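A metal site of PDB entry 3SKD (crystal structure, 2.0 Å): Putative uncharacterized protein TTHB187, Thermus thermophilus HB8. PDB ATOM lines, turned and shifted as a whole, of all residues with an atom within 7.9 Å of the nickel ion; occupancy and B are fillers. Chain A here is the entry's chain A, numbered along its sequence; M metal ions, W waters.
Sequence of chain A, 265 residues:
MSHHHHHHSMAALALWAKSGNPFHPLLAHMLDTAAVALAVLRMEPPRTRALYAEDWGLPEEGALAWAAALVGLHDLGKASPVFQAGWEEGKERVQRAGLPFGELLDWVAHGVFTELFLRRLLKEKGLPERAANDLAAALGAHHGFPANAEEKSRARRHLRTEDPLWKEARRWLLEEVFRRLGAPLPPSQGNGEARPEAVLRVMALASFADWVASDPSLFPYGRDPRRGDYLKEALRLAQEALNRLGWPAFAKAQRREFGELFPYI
Ser 214 touches the nickel ion.
Water W1 bridges OD1 of Asp 75 (2.7 Å) and NE2 of His 110 (3.5 Å).
Water W2 binds the nickel ion, 2.0 Å away.
The nickel ion is bound by OD2 of Asp 75 (2.0 Å).
OD1 of Asp 210 binds the nickel ion, 2.2 Å away.
The nickel ion is bound by NE2 of His 74, 2.3 Å away.
A ring nitrogen (NE2) of His 29 binds the nickel ion, 2.3 Å away.
The nickel ion is bound by water W1 (2.4 Å).
The nickel ion has six donor atoms within binding distance.
The side-chain amino group (NZ) of Lys 78 sits close to the side-chain carboxylate (OD2) of Asp 75 (3.1 Å).
A ring nitrogen (NE2) of His 110 lies within hydrogen-bond range of the side-chain carboxylate of Asp 75 (2.9 Å).
OG of Ser 214 lies within hydrogen-bond range of O of Asp 210, 2.6 Å away.
O of Val 71 is in hydrogen-bond range of ND1 of His 74, 3.0 Å away.
The backbone carbonyl oxygen of His 29 sits at hydrogen-bond distance from the side-chain hydroxyl of Thr 33, 2.9 Å away.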
ATOM      1  N   SER A  19     -19.276 -30.226  -8.845  1.00  0.00           N
ATOM      2  CA  SER A  19     -18.055 -29.818  -9.526  1.00  0.00           C
ATOM      3  C   SER A  19     -17.981 -30.353 -10.950  1.00  0.00           C
ATOM      4  O   SER A  19     -17.822 -31.537 -11.146  1.00  0.00           O
ATOM      5  CB  SER A  19     -16.827 -30.289  -8.746  1.00  0.00           C
ATOM      6  OG  SER A  19     -15.666 -29.693  -9.300  1.00  0.00           O
ATOM      7  N   LEU A  26     -19.024 -31.883  -5.643  1.00  0.00           N
ATOM      8  CA  LEU A  26     -17.795 -31.202  -5.250  1.00  0.00           C
ATOM      9  C   LEU A  26     -16.978 -32.084  -4.304  1.00  0.00           C
ATOM     10  O   LEU A  26     -15.766 -32.214  -4.461  1.00  0.00           O
ATOM     11  CB  LEU A  26     -18.144 -29.863  -4.609  1.00  0.00           C
ATOM     12  CG  LEU A  26     -16.958 -28.989  -4.179  1.00  0.00           C
ATOM     13  CD1 LEU A  26     -15.976 -28.792  -5.284  1.00  0.00           C
ATOM     14  CD2 LEU A  26     -17.445 -27.658  -3.640  1.00  0.00           C
ATOM     15  N   HIS A  29     -15.051 -34.660  -6.217  1.00  0.00           N
ATOM     16  CA  HIS A  29     -13.892 -34.118  -6.868  1.00  0.00           C
ATOM     17  C   HIS A  29     -12.781 -33.764  -5.854  1.00  0.00           C
ATOM     18  O   HIS A  29     -11.593 -33.952  -6.122  1.00  0.00           O
ATOM     19  CB  HIS A  29     -14.267 -32.875  -7.635  1.00  0.00           C
ATOM     20  CG  HIS A  29     -13.099 -32.203  -8.256  1.00  0.00           C
ATOM     21  ND1 HIS A  29     -12.210 -32.865  -9.076  1.00  0.00           N
ATOM     22  CD2 HIS A  29     -12.633 -30.925  -8.145  1.00  0.00           C
ATOM     23  CE1 HIS A  29     -11.274 -32.032  -9.462  1.00  0.00           C
ATOM     24  NE2 HIS A  29     -11.507 -30.863  -8.911  1.00  0.00           N
ATOM     25  N   MET A  30     -13.153 -33.301  -4.673  1.00  0.00           N
ATOM     26  CA  MET A  30     -12.156 -32.934  -3.658  1.00  0.00           C
ATOM     27  C   MET A  30     -11.412 -34.172  -3.190  1.00  0.00           C
ATOM     28  O   MET A  30     -10.163 -34.180  -3.058  1.00  0.00           O
ATOM     29  CB  MET A  30     -12.758 -32.204  -2.454  1.00  0.00           C
ATOM     30  CG  MET A  30     -13.188 -30.709  -2.704  1.00  0.00           C
ATOM     31  SD  MET A  30     -14.287 -30.141  -1.308  1.00  0.00           S
ATOM     32  CE  MET A  30     -13.169 -30.098   0.059  1.00  0.00           C
ATOM     33  N   THR A  33      -9.060 -35.469  -6.013  1.00  0.00           N
ATOM     34  CA  THR A  33      -7.887 -34.610  -6.081  1.00  0.00           C
ATOM     35  C   THR A  33      -6.894 -34.993  -4.939  1.00  0.00           C
ATOM     36  O   THR A  33      -5.703 -35.225  -5.192  1.00  0.00           O
ATOM     37  CB  THR A  33      -8.314 -33.119  -6.096  1.00  0.00           C
ATOM     38  OG1 THR A  33      -9.140 -32.887  -7.260  1.00  0.00           O
ATOM     39  CG2 THR A  33      -7.057 -32.149  -6.161  1.00  0.00           C
ATOM     40  N   VAL A  71      -4.521 -30.142  -0.675  1.00  0.00           N
ATOM     41  CA  VAL A  71      -4.657 -30.097  -2.112  1.00  0.00           C
ATOM     42  C   VAL A  71      -6.106 -30.463  -2.517  1.00  0.00           C
ATOM     43  O   VAL A  71      -6.665 -29.897  -3.455  1.00  0.00           O
ATOM     44  CB  VAL A  71      -3.648 -31.029  -2.666  1.00  0.00           C
ATOM     45  CG1 VAL A  71      -3.980 -31.420  -4.024  1.00  0.00           C
ATOM     46  CG2 VAL A  71      -2.200 -30.335  -2.545  1.00  0.00           C
ATOM     47  N   GLY A  72      -6.707 -31.373  -1.787  1.00  0.00           N
ATOM     48  CA  GLY A  72      -8.101 -31.679  -2.047  1.00  0.00           C
ATOM     49  C   GLY A  72      -9.004 -30.458  -1.887  1.00  0.00           C
ATOM     50  O   GLY A  72     -10.059 -30.399  -2.512  1.00  0.00           O
ATOM     51  N   LEU A  73      -8.629 -29.513  -1.019  1.00  0.00           N
ATOM     52  CA  LEU A  73      -9.485 -28.363  -0.755  1.00  0.00           C
ATOM     53  C   LEU A  73      -9.314 -27.249  -1.782  1.00  0.00           C
ATOM     54  O   LEU A  73      -9.840 -26.165  -1.563  1.00  0.00           O
ATOM     55  CB  LEU A  73      -9.146 -27.735   0.572  1.00  0.00           C
ATOM     56  CG  LEU A  73      -9.152 -28.684   1.762  1.00  0.00           C
ATOM     57  CD1 LEU A  73      -8.607 -27.888   2.933  1.00  0.00           C
ATOM     58  CD2 LEU A  73     -10.542 -29.164   1.966  1.00  0.00           C
ATOM     59  N   HIS A  74      -8.541 -27.466  -2.832  1.00  0.00           N
ATOM     60  CA  HIS A  74      -8.278 -26.393  -3.811  1.00  0.00           C
ATOM     61  C   HIS A  74      -9.572 -25.823  -4.416  1.00  0.00           C
ATOM     62  O   HIS A  74      -9.567 -24.699  -4.901  1.00  0.00           O
ATOM     63  CB  HIS A  74      -7.425 -26.889  -4.966  1.00  0.00           C
ATOM     64  CG  HIS A  74      -8.185 -27.754  -5.921  1.00  0.00           C
ATOM     65  ND1 HIS A  74      -8.574 -29.050  -5.612  1.00  0.00           N
ATOM     66  CD2 HIS A  74      -8.663 -27.515  -7.174  1.00  0.00           C
ATOM     67  CE1 HIS A  74      -9.250 -29.567  -6.636  1.00  0.00           C
ATOM     68  NE2 HIS A  74      -9.292 -28.653  -7.597  1.00  0.00           N
ATOM     69  N   ASP A  75     -10.627 -26.623  -4.488  1.00  0.00           N
ATOM     70  CA  ASP A  75     -11.906 -26.121  -5.055  1.00  0.00           C
ATOM     71  C   ASP A  75     -12.973 -25.828  -4.037  1.00  0.00           C
ATOM     72  O   ASP A  75     -14.153 -25.746  -4.378  1.00  0.00           O
ATOM     73  CB  ASP A  75     -12.530 -27.122  -6.048  1.00  0.00           C
ATOM     74  CG  ASP A  75     -11.941 -27.008  -7.460  1.00  0.00           C
ATOM     75  OD1 ASP A  75     -11.271 -25.990  -7.762  1.00  0.00           O
ATOM     76  OD2 ASP A  75     -12.083 -27.897  -8.277  1.00  0.00           O
ATOM     77  N   LEU A  76     -12.570 -25.627  -2.794  1.00  0.00           N
ATOM     78  CA  LEU A  76     -13.530 -25.237  -1.798  1.00  0.00           C
ATOM     79  C   LEU A  76     -14.288 -23.913  -2.205  1.00  0.00           C
ATOM     80  O   LEU A  76     -15.477 -23.750  -1.885  1.00  0.00           O
ATOM     81  CB  LEU A  76     -12.816 -25.092  -0.472  1.00  0.00           C
ATOM     82  CG  LEU A  76     -13.776 -24.776   0.642  1.00  0.00           C
ATOM     83  CD1 LEU A  76     -14.656 -26.000   0.777  1.00  0.00           C
ATOM     84  CD2 LEU A  76     -13.015 -24.486   1.892  1.00  0.00           C
ATOM     85  N   LYS A  78     -15.732 -23.259  -4.832  1.00  0.00           N
ATOM     86  CA  LYS A  78     -16.963 -23.615  -5.589  1.00  0.00           C
ATOM     87  C   LYS A  78     -18.195 -23.850  -4.702  1.00  0.00           C
ATOM     88  O   LYS A  78     -19.326 -23.933  -5.204  1.00  0.00           O
ATOM     89  CB  LYS A  78     -16.730 -24.872  -6.427  1.00  0.00           C
ATOM     90  CG  LYS A  78     -15.831 -24.661  -7.628  1.00  0.00           C
ATOM     91  CD  LYS A  78     -15.877 -25.871  -8.584  1.00  0.00           C
ATOM     92  CE  LYS A  78     -14.841 -25.740  -9.706  1.00  0.00           C
ATOM     93  NZ  LYS A  78     -14.369 -27.093 -10.184  1.00  0.00           N
ATOM     94  N   HIS A 110     -13.231 -18.952  -9.103  1.00  0.00           N
ATOM     95  CA  HIS A 110     -13.475 -19.698  -7.886  1.00  0.00           C
ATOM     96  C   HIS A 110     -12.249 -19.738  -6.952  1.00  0.00           C
ATOM     97  O   HIS A 110     -12.433 -19.822  -5.754  1.00  0.00           O
ATOM     98  CB  HIS A 110     -13.987 -21.097  -8.187  1.00  0.00           C
ATOM     99  CG  HIS A 110     -12.966 -22.027  -8.770  1.00  0.00           C
ATOM    100  ND1 HIS A 110     -12.759 -22.161 -10.128  1.00  0.00           N
ATOM    101  CD2 HIS A 110     -12.094 -22.866  -8.165  1.00  0.00           C
ATOM    102  CE1 HIS A 110     -11.775 -23.033 -10.335  1.00  0.00           C
ATOM    103  NE2 HIS A 110     -11.378 -23.489  -9.167  1.00  0.00           N
ATOM    104  N   ALA A 206      -1.009 -29.138  -6.144  1.00  0.00           N
ATOM    105  CA  ALA A 206      -2.477 -28.969  -6.284  1.00  0.00           C
ATOM    106  C   ALA A 206      -2.817 -28.745  -7.748  1.00  0.00           C
ATOM    107  O   ALA A 206      -3.736 -29.331  -8.274  1.00  0.00           O
ATOM    108  CB  ALA A 206      -2.966 -27.812  -5.456  1.00  0.00           C
ATOM    109  N   ALA A 209      -2.527 -32.153  -9.392  1.00  0.00           N
ATOM    110  CA  ALA A 209      -3.509 -33.164  -8.977  1.00  0.00           C
ATOM    111  C   ALA A 209      -4.901 -32.761  -9.451  1.00  0.00           C
ATOM    112  O   ALA A 209      -5.722 -33.587  -9.799  1.00  0.00           O
ATOM    113  CB  ALA A 209      -3.522 -33.317  -7.503  1.00  0.00           C
ATOM    114  N   ASP A 210      -5.152 -31.462  -9.421  1.00  0.00           N
ATOM    115  CA  ASP A 210      -6.439 -30.924  -9.901  1.00  0.00           C
ATOM    116  C   ASP A 210      -6.644 -31.235 -11.368  1.00  0.00           C
ATOM    117  O   ASP A 210      -7.721 -31.640 -11.803  1.00  0.00           O
ATOM    118  CB  ASP A 210      -6.516 -29.445  -9.658  1.00  0.00           C
ATOM    119  CG  ASP A 210      -7.849 -28.847 -10.170  1.00  0.00           C
ATOM    120  OD1 ASP A 210      -8.831 -29.591 -10.378  1.00  0.00           O
ATOM    121  OD2 ASP A 210      -7.954 -27.626 -10.284  1.00  0.00           O
ATOM    122  N   TRP A 211      -5.574 -31.121 -12.117  1.00  0.00           N
ATOM    123  CA  TRP A 211      -5.623 -31.466 -13.516  1.00  0.00           C
ATOM    124  C   TRP A 211      -5.899 -32.927 -13.775  1.00  0.00           C
ATOM    125  O   TRP A 211      -6.733 -33.275 -14.644  1.00  0.00           O
ATOM    126  CB  TRP A 211      -4.280 -31.081 -14.084  1.00  0.00           C
ATOM    127  CG  TRP A 211      -4.162 -31.391 -15.461  1.00  0.00           C
ATOM    128  CD1 TRP A 211      -4.857 -30.805 -16.483  1.00  0.00           C
ATOM    129  CD2 TRP A 211      -3.331 -32.376 -16.037  1.00  0.00           C
ATOM    130  NE1 TRP A 211      -4.486 -31.361 -17.656  1.00  0.00           N
ATOM    131  CE2 TRP A 211      -3.555 -32.330 -17.437  1.00  0.00           C
ATOM    132  CE3 TRP A 211      -2.399 -33.279 -15.529  1.00  0.00           C
ATOM    133  CZ2 TRP A 211      -2.879 -33.134 -18.318  1.00  0.00           C
ATOM    134  CZ3 TRP A 211      -1.728 -34.111 -16.419  1.00  0.00           C
ATOM    135  CH2 TRP A 211      -1.983 -34.034 -17.806  1.00  0.00           C
ATOM    136  N   ALA A 213      -7.355 -35.101 -11.714  1.00  0.00           N
ATOM    137  CA  ALA A 213      -8.668 -35.488 -11.192  1.00  0.00           C
ATOM    138  C   ALA A 213      -9.828 -34.895 -11.992  1.00  0.00           C
ATOM    139  O   ALA A 213     -10.943 -35.412 -11.936  1.00  0.00           O
ATOM    140  CB  ALA A 213      -8.802 -35.042  -9.800  1.00  0.00           C
ATOM    141  N   SER A 214      -9.535 -33.832 -12.732  1.00  0.00           N
ATOM    142  CA  SER A 214     -10.554 -33.095 -13.472  1.00  0.00           C
ATOM    143  C   SER A 214     -10.888 -33.789 -14.793  1.00  0.00           C
ATOM    144  O   SER A 214     -11.812 -33.379 -15.490  1.00  0.00           O
ATOM    145  CB  SER A 214     -10.109 -31.650 -13.735  1.00  0.00           C
ATOM    146  OG  SER A 214     -10.166 -30.903 -12.509  1.00  0.00           O
HETATM  147 NI    NI M   1     -10.659 -28.761  -9.393  1.00  0.00          NI
HETATM  148  O   HOH W   1     -10.063 -26.587 -10.072  1.00  0.00           O
HETATM  149  O   HOH W   2     -11.545 -29.019 -11.152  1.00  0.00           O
